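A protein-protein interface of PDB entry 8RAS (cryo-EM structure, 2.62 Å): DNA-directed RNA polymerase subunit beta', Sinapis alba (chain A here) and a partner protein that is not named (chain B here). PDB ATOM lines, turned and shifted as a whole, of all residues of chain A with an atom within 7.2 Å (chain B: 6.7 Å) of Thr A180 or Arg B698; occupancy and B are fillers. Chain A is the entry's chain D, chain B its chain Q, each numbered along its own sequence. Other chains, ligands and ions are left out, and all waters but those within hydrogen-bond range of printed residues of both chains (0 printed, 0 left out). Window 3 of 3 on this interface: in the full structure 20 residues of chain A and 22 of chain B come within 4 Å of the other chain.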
ATOM      1  N   SER A 174     -14.561 -13.501   2.800  1.00  0.00           N
ATOM      2  CA  SER A 174     -14.067 -12.218   3.293  1.00  0.00           C
ATOM      3  C   SER A 174     -14.108 -11.147   2.210  1.00  0.00           C
ATOM      4  O   SER A 174     -14.825 -10.148   2.333  1.00  0.00           O
ATOM      5  CB  SER A 174     -12.645 -12.387   3.834  1.00  0.00           C
ATOM      6  OG  SER A 174     -12.525 -13.578   4.590  1.00  0.00           O
ATOM      7  N   ILE A 175     -13.349 -11.341   1.137  1.00  0.00           N
ATOM      8  CA  ILE A 175     -13.261 -10.350   0.067  1.00  0.00           C
ATOM      9  C   ILE A 175     -14.625 -10.120  -0.583  1.00  0.00           C
ATOM     10  O   ILE A 175     -15.027  -8.957  -0.735  1.00  0.00           O
ATOM     11  CB  ILE A 175     -12.205 -10.750  -0.976  1.00  0.00           C
ATOM     12  CG1 ILE A 175     -10.800 -10.644  -0.380  1.00  0.00           C
ATOM     13  CG2 ILE A 175     -12.316  -9.866  -2.204  1.00  0.00           C
ATOM     14  CD1 ILE A 175     -10.247 -11.955   0.123  1.00  0.00           C
ATOM     15  N   PRO A 176     -15.376 -11.158  -0.986  1.00  0.00           N
ATOM     16  CA  PRO A 176     -16.700 -10.886  -1.574  1.00  0.00           C
ATOM     17  C   PRO A 176     -17.659 -10.184  -0.629  1.00  0.00           C
ATOM     18  O   PRO A 176     -18.433  -9.326  -1.068  1.00  0.00           O
ATOM     19  CB  PRO A 176     -17.209 -12.282  -1.960  1.00  0.00           C
ATOM     20  CG  PRO A 176     -16.000 -13.120  -2.055  1.00  0.00           C
ATOM     21  CD  PRO A 176     -15.071 -12.602  -1.011  1.00  0.00           C
ATOM     22  N   LEU A 177     -17.632 -10.515   0.662  1.00  0.00           N
ATOM     23  CA  LEU A 177     -18.584  -9.904   1.584  1.00  0.00           C
ATOM     24  C   LEU A 177     -18.217  -8.459   1.898  1.00  0.00           C
ATOM     25  O   LEU A 177     -19.107  -7.640   2.153  1.00  0.00           O
ATOM     26  CB  LEU A 177     -18.679 -10.731   2.868  1.00  0.00           C
ATOM     27  CG  LEU A 177     -19.925 -10.539   3.730  1.00  0.00           C
ATOM     28  CD1 LEU A 177     -21.157 -11.039   2.995  1.00  0.00           C
ATOM     29  CD2 LEU A 177     -19.765 -11.279   5.046  1.00  0.00           C
ATOM     30  N   PHE A 178     -16.925  -8.129   1.885  1.00  0.00           N
ATOM     31  CA  PHE A 178     -16.511  -6.739   2.034  1.00  0.00           C
ATOM     32  C   PHE A 178     -16.723  -5.953   0.745  1.00  0.00           C
ATOM     33  O   PHE A 178     -17.052  -4.762   0.787  1.00  0.00           O
ATOM     34  CB  PHE A 178     -15.046  -6.667   2.466  1.00  0.00           C
ATOM     35  CG  PHE A 178     -14.459  -5.286   2.387  1.00  0.00           C
ATOM     36  CD1 PHE A 178     -14.813  -4.314   3.308  1.00  0.00           C
ATOM     37  CD2 PHE A 178     -13.554  -4.960   1.391  1.00  0.00           C
ATOM     38  CE1 PHE A 178     -14.273  -3.042   3.236  1.00  0.00           C
ATOM     39  CE2 PHE A 178     -13.013  -3.691   1.313  1.00  0.00           C
ATOM     40  CZ  PHE A 178     -13.373  -2.732   2.237  1.00  0.00           C
ATOM     41  N   PHE A 179     -16.543  -6.601  -0.404  1.00  0.00           N
ATOM     42  CA  PHE A 179     -16.650  -5.952  -1.702  1.00  0.00           C
ATOM     43  C   PHE A 179     -18.026  -6.113  -2.338  1.00  0.00           C
ATOM     44  O   PHE A 179     -18.186  -5.787  -3.518  1.00  0.00           O
ATOM     45  CB  PHE A 179     -15.582  -6.497  -2.656  1.00  0.00           C
ATOM     46  CG  PHE A 179     -14.234  -5.859  -2.491  1.00  0.00           C
ATOM     47  CD1 PHE A 179     -13.958  -4.630  -3.069  1.00  0.00           C
ATOM     48  CD2 PHE A 179     -13.238  -6.490  -1.767  1.00  0.00           C
ATOM     49  CE1 PHE A 179     -12.718  -4.044  -2.920  1.00  0.00           C
ATOM     50  CE2 PHE A 179     -11.995  -5.910  -1.616  1.00  0.00           C
ATOM     51  CZ  PHE A 179     -11.734  -4.686  -2.194  1.00  0.00           C
ATOM     52  N   THR A 180     -19.011  -6.611  -1.587  1.00  0.00           N
ATOM     53  CA  THR A 180     -20.352  -6.890  -2.096  1.00  0.00           C
ATOM     54  C   THR A 180     -20.300  -7.843  -3.284  1.00  0.00           C
ATOM     55  O   THR A 180     -19.310  -8.552  -3.475  1.00  0.00           O
ATOM     56  CB  THR A 180     -21.086  -5.599  -2.477  1.00  0.00           C
ATOM     57  OG1 THR A 180     -20.421  -4.961  -3.575  1.00  0.00           O
ATOM     58  CG2 THR A 180     -21.140  -4.647  -1.289  1.00  0.00           C
ATOM     59  N   THR A 181     -21.361  -7.875  -4.087  1.00  0.00           N
ATOM     60  CA  THR A 181     -21.479  -8.848  -5.165  1.00  0.00           C
ATOM     61  C   THR A 181     -21.288  -8.245  -6.549  1.00  0.00           C
ATOM     62  O   THR A 181     -20.521  -8.785  -7.350  1.00  0.00           O
ATOM     63  CB  THR A 181     -22.842  -9.550  -5.092  1.00  0.00           C
ATOM     64  OG1 THR A 181     -23.883  -8.608  -5.379  1.00  0.00           O
ATOM     65  CG2 THR A 181     -23.060 -10.137  -3.706  1.00  0.00           C
ATOM     66  N   GLN A 182     -21.971  -7.140  -6.856  1.00  0.00           N
ATOM     67  CA  GLN A 182     -21.926  -6.600  -8.213  1.00  0.00           C
ATOM     68  C   GLN A 182     -20.521  -6.135  -8.582  1.00  0.00           C
ATOM     69  O   GLN A 182     -19.965  -6.556  -9.602  1.00  0.00           O
ATOM     70  CB  GLN A 182     -22.929  -5.454  -8.352  1.00  0.00           C
ATOM     71  CG  GLN A 182     -24.376  -5.877  -8.170  1.00  0.00           C
ATOM     72  CD  GLN A 182     -25.335  -4.704  -8.207  1.00  0.00           C
ATOM     73  OE1 GLN A 182     -24.955  -3.567  -7.925  1.00  0.00           O
ATOM     74  NE2 GLN A 182     -26.587  -4.974  -8.557  1.00  0.00           N
ATOM     75  N   GLY A 183     -19.920  -5.284  -7.750  1.00  0.00           N
ATOM     76  CA  GLY A 183     -18.580  -4.802  -8.047  1.00  0.00           C
ATOM     77  C   GLY A 183     -17.540  -5.905  -7.986  1.00  0.00           C
ATOM     78  O   GLY A 183     -16.611  -5.946  -8.801  1.00  0.00           O
ATOM     79  N   PHE A 184     -17.685  -6.815  -7.019  1.00  0.00           N
ATOM     80  CA  PHE A 184     -16.756  -7.932  -6.907  1.00  0.00           C
ATOM     81  C   PHE A 184     -16.779  -8.791  -8.162  1.00  0.00           C
ATOM     82  O   PHE A 184     -15.722  -9.158  -8.686  1.00  0.00           O
ATOM     83  CB  PHE A 184     -17.088  -8.768  -5.672  1.00  0.00           C
ATOM     84  CG  PHE A 184     -16.268 -10.019  -5.546  1.00  0.00           C
ATOM     85  CD1 PHE A 184     -15.009  -9.983  -4.974  1.00  0.00           C
ATOM     86  CD2 PHE A 184     -16.765 -11.236  -5.982  1.00  0.00           C
ATOM     87  CE1 PHE A 184     -14.256 -11.132  -4.853  1.00  0.00           C
ATOM     88  CE2 PHE A 184     -16.016 -12.387  -5.862  1.00  0.00           C
ATOM     89  CZ  PHE A 184     -14.761 -12.336  -5.296  1.00  0.00           C
ATOM     90  N   GLU A 185     -17.972  -9.107  -8.670  1.00  0.00           N
ATOM     91  CA  GLU A 185     -18.070  -9.852  -9.919  1.00  0.00           C
ATOM     92  C   GLU A 185     -17.573  -9.031 -11.101  1.00  0.00           C
ATOM     93  O   GLU A 185     -17.055  -9.596 -12.071  1.00  0.00           O
ATOM     94  CB  GLU A 185     -19.511 -10.305 -10.151  1.00  0.00           C
ATOM     95  CG  GLU A 185     -19.958 -11.439  -9.242  1.00  0.00           C
ATOM     96  CD  GLU A 185     -19.261 -12.747  -9.555  1.00  0.00           C
ATOM     97  OE1 GLU A 185     -19.120 -13.075 -10.752  1.00  0.00           O
ATOM     98  OE2 GLU A 185     -18.853 -13.448  -8.606  1.00  0.00           O
ATOM     99  N   PHE A 187     -15.002  -6.948 -11.072  1.00  0.00           N
ATOM    100  CA  PHE A 187     -13.551  -7.101 -11.077  1.00  0.00           C
ATOM    101  C   PHE A 187     -13.108  -8.531 -10.777  1.00  0.00           C
ATOM    102  O   PHE A 187     -11.905  -8.789 -10.678  1.00  0.00           O
ATOM    103  CB  PHE A 187     -12.909  -6.086 -10.111  1.00  0.00           C
ATOM    104  CG  PHE A 187     -12.785  -6.552  -8.676  1.00  0.00           C
ATOM    105  CD1 PHE A 187     -11.686  -7.285  -8.249  1.00  0.00           C
ATOM    106  CD2 PHE A 187     -13.750  -6.216  -7.745  1.00  0.00           C
ATOM    107  CE1 PHE A 187     -11.570  -7.698  -6.936  1.00  0.00           C
ATOM    108  CE2 PHE A 187     -13.635  -6.624  -6.428  1.00  0.00           C
ATOM    109  CZ  PHE A 187     -12.545  -7.367  -6.026  1.00  0.00           C
ATOM    110  N   THR B 646      -7.706   6.903 -10.004  1.00  0.00           N
ATOM    111  CA  THR B 646      -8.862   6.366 -10.712  1.00  0.00           C
ATOM    112  C   THR B 646      -9.389   7.452 -11.644  1.00  0.00           C
ATOM    113  O   THR B 646      -8.709   8.449 -11.909  1.00  0.00           O
ATOM    114  CB  THR B 646      -9.944   5.882  -9.740  1.00  0.00           C
ATOM    115  OG1 THR B 646     -11.064   5.397 -10.489  1.00  0.00           O
ATOM    116  CG2 THR B 646     -10.400   7.017  -8.839  1.00  0.00           C
ATOM    117  N   ASP B 695      -8.201   1.144 -12.069  1.00  0.00           N
ATOM    118  CA  ASP B 695      -9.012   1.730 -13.134  1.00  0.00           C
ATOM    119  C   ASP B 695     -10.385   2.158 -12.631  1.00  0.00           C
ATOM    120  O   ASP B 695     -10.869   3.240 -12.984  1.00  0.00           O
ATOM    121  CB  ASP B 695      -9.149   0.744 -14.294  1.00  0.00           C
ATOM    122  CG  ASP B 695      -9.352  -0.680 -13.826  1.00  0.00           C
ATOM    123  OD1 ASP B 695     -10.235  -1.369 -14.379  1.00  0.00           O
ATOM    124  OD2 ASP B 695      -8.635  -1.109 -12.900  1.00  0.00           O
ATOM    125  N   VAL B 696     -11.025   1.332 -11.810  1.00  0.00           N
ATOM    126  CA  VAL B 696     -12.381   1.589 -11.338  1.00  0.00           C
ATOM    127  C   VAL B 696     -12.310   2.203  -9.947  1.00  0.00           C
ATOM    128  O   VAL B 696     -11.577   1.714  -9.077  1.00  0.00           O
ATOM    129  CB  VAL B 696     -13.226   0.301 -11.343  1.00  0.00           C
ATOM    130  CG1 VAL B 696     -12.470  -0.845 -10.689  1.00  0.00           C
ATOM    131  CG2 VAL B 696     -14.565   0.535 -10.659  1.00  0.00           C
ATOM    132  N   ARG B 697     -13.063   3.287  -9.743  1.00  0.00           N
ATOM    133  CA  ARG B 697     -13.037   4.004  -8.473  1.00  0.00           C
ATOM    134  C   ARG B 697     -13.553   3.161  -7.316  1.00  0.00           C
ATOM    135  O   ARG B 697     -13.237   3.461  -6.159  1.00  0.00           O
ATOM    136  CB  ARG B 697     -13.866   5.284  -8.581  1.00  0.00           C
ATOM    137  CG  ARG B 697     -15.352   5.070  -8.332  1.00  0.00           C
ATOM    138  CD  ARG B 697     -16.208   6.028  -9.137  1.00  0.00           C
ATOM    139  NE  ARG B 697     -15.989   5.888 -10.572  1.00  0.00           N
ATOM    140  CZ  ARG B 697     -15.510   6.847 -11.349  1.00  0.00           C
ATOM    141  NH1 ARG B 697     -15.185   8.033 -10.860  1.00  0.00           N
ATOM    142  NH2 ARG B 697     -15.355   6.614 -12.649  1.00  0.00           N
ATOM    143  N   ARG B 698     -14.332   2.117  -7.600  1.00  0.00           N
ATOM    144  CA  ARG B 698     -14.994   1.361  -6.543  1.00  0.00           C
ATOM    145  C   ARG B 698     -13.978   0.711  -5.608  1.00  0.00           C
ATOM    146  O   ARG B 698     -13.886   1.061  -4.425  1.00  0.00           O
ATOM    147  CB  ARG B 698     -15.912   0.312  -7.172  1.00  0.00           C
ATOM    148  CG  ARG B 698     -17.121  -0.039  -6.337  1.00  0.00           C
ATOM    149  CD  ARG B 698     -16.904  -1.346  -5.613  1.00  0.00           C
ATOM    150  NE  ARG B 698     -18.027  -1.683  -4.750  1.00  0.00           N
ATOM    151  CZ  ARG B 698     -18.026  -2.691  -3.891  1.00  0.00           C
ATOM    152  NH1 ARG B 698     -16.975  -3.482  -3.759  1.00  0.00           N
ATOM    153  NH2 ARG B 698     -19.106  -2.911  -3.148  1.00  0.00           N
ATOM    154  N   VAL B 699     -13.188  -0.227  -6.135  1.00  0.00           N
ATOM    155  CA  VAL B 699     -12.205  -0.921  -5.309  1.00  0.00           C
ATOM    156  C   VAL B 699     -11.148   0.049  -4.803  1.00  0.00           C
ATOM    157  O   VAL B 699     -10.607  -0.127  -3.705  1.00  0.00           O
ATOM    158  CB  VAL B 699     -11.580  -2.091  -6.098  1.00  0.00           C
ATOM    159  CG1 VAL B 699     -11.096  -1.621  -7.457  1.00  0.00           C
ATOM    160  CG2 VAL B 699     -10.446  -2.730  -5.313  1.00  0.00           C
ATOM    161  N   ALA B 700     -10.845   1.092  -5.580  1.00  0.00           N
ATOM    162  CA  ALA B 700      -9.864   2.080  -5.144  1.00  0.00           C
ATOM    163  C   ALA B 700     -10.304   2.758  -3.852  1.00  0.00           C
ATOM    164  O   ALA B 700      -9.540   2.825  -2.881  1.00  0.00           O
ATOM    165  CB  ALA B 700      -9.635   3.113  -6.247  1.00  0.00           C
ATOM    166  N   VAL B 701     -11.542   3.257  -3.813  1.00  0.00           N
ATOM    167  CA  VAL B 701     -12.010   3.916  -2.598  1.00  0.00           C
ATOM    168  C   VAL B 701     -12.242   2.903  -1.484  1.00  0.00           C
ATOM    169  O   VAL B 701     -12.096   3.237  -0.305  1.00  0.00           O
ATOM    170  CB  VAL B 701     -13.266   4.767  -2.871  1.00  0.00           C
ATOM    171  CG1 VAL B 701     -13.002   5.765  -3.989  1.00  0.00           C
ATOM    172  CG2 VAL B 701     -14.458   3.894  -3.193  1.00  0.00           C
ATOM    173  N   ARG B 702     -12.594   1.655  -1.820  1.00  0.00           N
ATOM    174  CA  ARG B 702     -12.705   0.638  -0.775  1.00  0.00           C
ATOM    175  C   ARG B 702     -11.363   0.413  -0.086  1.00  0.00           C
ATOM    176  O   ARG B 702     -11.286   0.366   1.149  1.00  0.00           O
ATOM    177  CB  ARG B 702     -13.233  -0.676  -1.355  1.00  0.00           C
ATOM    178  CG  ARG B 702     -14.607  -0.581  -1.999  1.00  0.00           C
ATOM    179  CD  ARG B 702     -15.672  -0.158  -1.006  1.00  0.00           C
ATOM    180  NE  ARG B 702     -16.360  -1.299  -0.416  1.00  0.00           N
ATOM    181  CZ  ARG B 702     -17.667  -1.510  -0.502  1.00  0.00           C
ATOM    182  NH1 ARG B 702     -18.460  -0.672  -1.149  1.00  0.00           N
ATOM    183  NH2 ARG B 702     -18.190  -2.587   0.075  1.00  0.00           N
ATOM    184  N   CYS B 703     -10.288   0.301  -0.868  1.00  0.00           N
ATOM    185  CA  CYS B 703      -8.959   0.129  -0.292  1.00  0.00           C
ATOM    186  C   CYS B 703      -8.511   1.382   0.450  1.00  0.00           C
ATOM    187  O   CYS B 703      -7.835   1.291   1.481  1.00  0.00           O
ATOM    188  CB  CYS B 703      -7.955  -0.236  -1.385  1.00  0.00           C
ATOM    189  SG  CYS B 703      -8.326  -1.770  -2.266  1.00  0.00           S
ATOM    190  N   TYR B 734     -24.648   6.020  -9.043  1.00  0.00           N
ATOM    191  CA  TYR B 734     -23.538   5.697  -8.156  1.00  0.00           C
ATOM    192  C   TYR B 734     -23.354   6.841  -7.172  1.00  0.00           C
ATOM    193  O   TYR B 734     -23.189   7.992  -7.585  1.00  0.00           O
ATOM    194  CB  TYR B 734     -22.248   5.458  -8.950  1.00  0.00           C
ATOM    195  CG  TYR B 734     -20.997   5.431  -8.100  1.00  0.00           C
ATOM    196  CD1 TYR B 734     -20.616   4.279  -7.427  1.00  0.00           C
ATOM    197  CD2 TYR B 734     -20.194   6.558  -7.975  1.00  0.00           C
ATOM    198  CE1 TYR B 734     -19.474   4.250  -6.650  1.00  0.00           C
ATOM    199  CE2 TYR B 734     -19.053   6.540  -7.200  1.00  0.00           C
ATOM    200  CZ  TYR B 734     -18.697   5.383  -6.542  1.00  0.00           C
ATOM    201  OH  TYR B 734     -17.559   5.359  -5.770  1.00  0.00           O
ATOM    202  N   GLU B 739     -21.261   4.607  -0.758  1.00  0.00           N
ATOM    203  CA  GLU B 739     -20.224   3.594  -0.914  1.00  0.00           C
ATOM    204  C   GLU B 739     -19.143   3.743   0.150  1.00  0.00           C
ATOM    205  O   GLU B 739     -18.636   2.743   0.673  1.00  0.00           O
ATOM    206  CB  GLU B 739     -19.618   3.670  -2.312  1.00  0.00           C
ATOM    207  CG  GLU B 739     -18.849   2.424  -2.703  1.00  0.00           C
ATOM    208  CD  GLU B 739     -17.677   2.726  -3.606  1.00  0.00           C
ATOM    209  OE1 GLU B 739     -17.585   3.871  -4.097  1.00  0.00           O
ATOM    210  OE2 GLU B 739     -16.842   1.824  -3.814  1.00  0.00           O
ATOM    211  N   GLU B 742     -20.563   2.257   3.273  1.00  0.00           N
ATOM    212  CA  GLU B 742     -20.493   0.800   3.249  1.00  0.00           C
ATOM    213  C   GLU B 742     -19.071   0.308   3.493  1.00  0.00           C
ATOM    214  O   GLU B 742     -18.860  -0.673   4.216  1.00  0.00           O
ATOM    215  CB  GLU B 742     -21.021   0.269   1.915  1.00  0.00           C
ATOM    216  CG  GLU B 742     -22.509   0.484   1.706  1.00  0.00           C
ATOM    217  CD  GLU B 742     -22.904   0.428   0.245  1.00  0.00           C
ATOM    218  OE1 GLU B 742     -22.777   1.459  -0.447  1.00  0.00           O
ATOM    219  OE2 GLU B 742     -23.342  -0.648  -0.211  1.00  0.00           O
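OG1 of Thr A180 lies within hydrogen-bond range of NH2 of Arg B698 (2.5 Å).
O of Phe A178 is in hydrogen-bond range of NH2 of Arg B702, 2.6 Å away.
NH1 of Arg B698 sits at hydrogen-bond distance from O of Phe A179, 2.6 Å away.
The guanidinium group (NH1) of Arg B702 lies within salt-bridge range of the side-chain carboxylate (OE2) of Glu B739.
The backbone carbonyl oxygen (O) of Val B699 lies within hydrogen-bond range of the side-chain sulfur (SG) of Cys B703.
The side-chain carboxylate (OE2) of Glu B739 lies within salt-bridge range of the guanidinium group (NE) of Arg B698 (3.8 Å).
CG2 of Val B699 touches CE1 of Phe A179, 3.6 Å away.
CE1 of Phe A179 touches CB of Arg B702 (3.7 Å).
CG2 of Thr A180 touches NH2 of Arg B702 (3.8 Å).
Of chain B, only Arg B698 (2.5 Å) and Arg B702 (3.8 Å) come within 4 Å of Thr A180.
Of chain A, only Phe A179 (2.6 Å) and Thr A180 (2.5 Å) come within 4 Å of Arg B698.
Printed residues of chain B within 4 Å of Phe A178: Arg B702 (2.6 Å).
Printed residues of chain A within 4 Å of Val B699: Phe A179 (3.6 Å).
Printed residues of chain B within 4 Å of Phe A179: Arg B698 (2.6 Å), Val B699 (3.6 Å) and Arg B702 (3.7 Å).
Of the printed residues of chain A, Arg B702 touches Phe A178, Phe A179 and Thr A180.
Phe A184 touches none of the printed residues of chain B.
Glu B739 touches none of the printed residues of chain A.
The nearest residue of chain B that does not touch Thr A180 is Glu B742 (4.7 Å).
The nearest residue of chain A that does not touch Arg B698 is Gly A183 (4.5 Å).
Of the 13 printed residues of chain B, 3 touch a printed residue of chain A.
Among the printed residues, no Asp or Glu carboxylate lies within 4 Å of a Lys or Arg side-chain nitrogen of the other chain.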
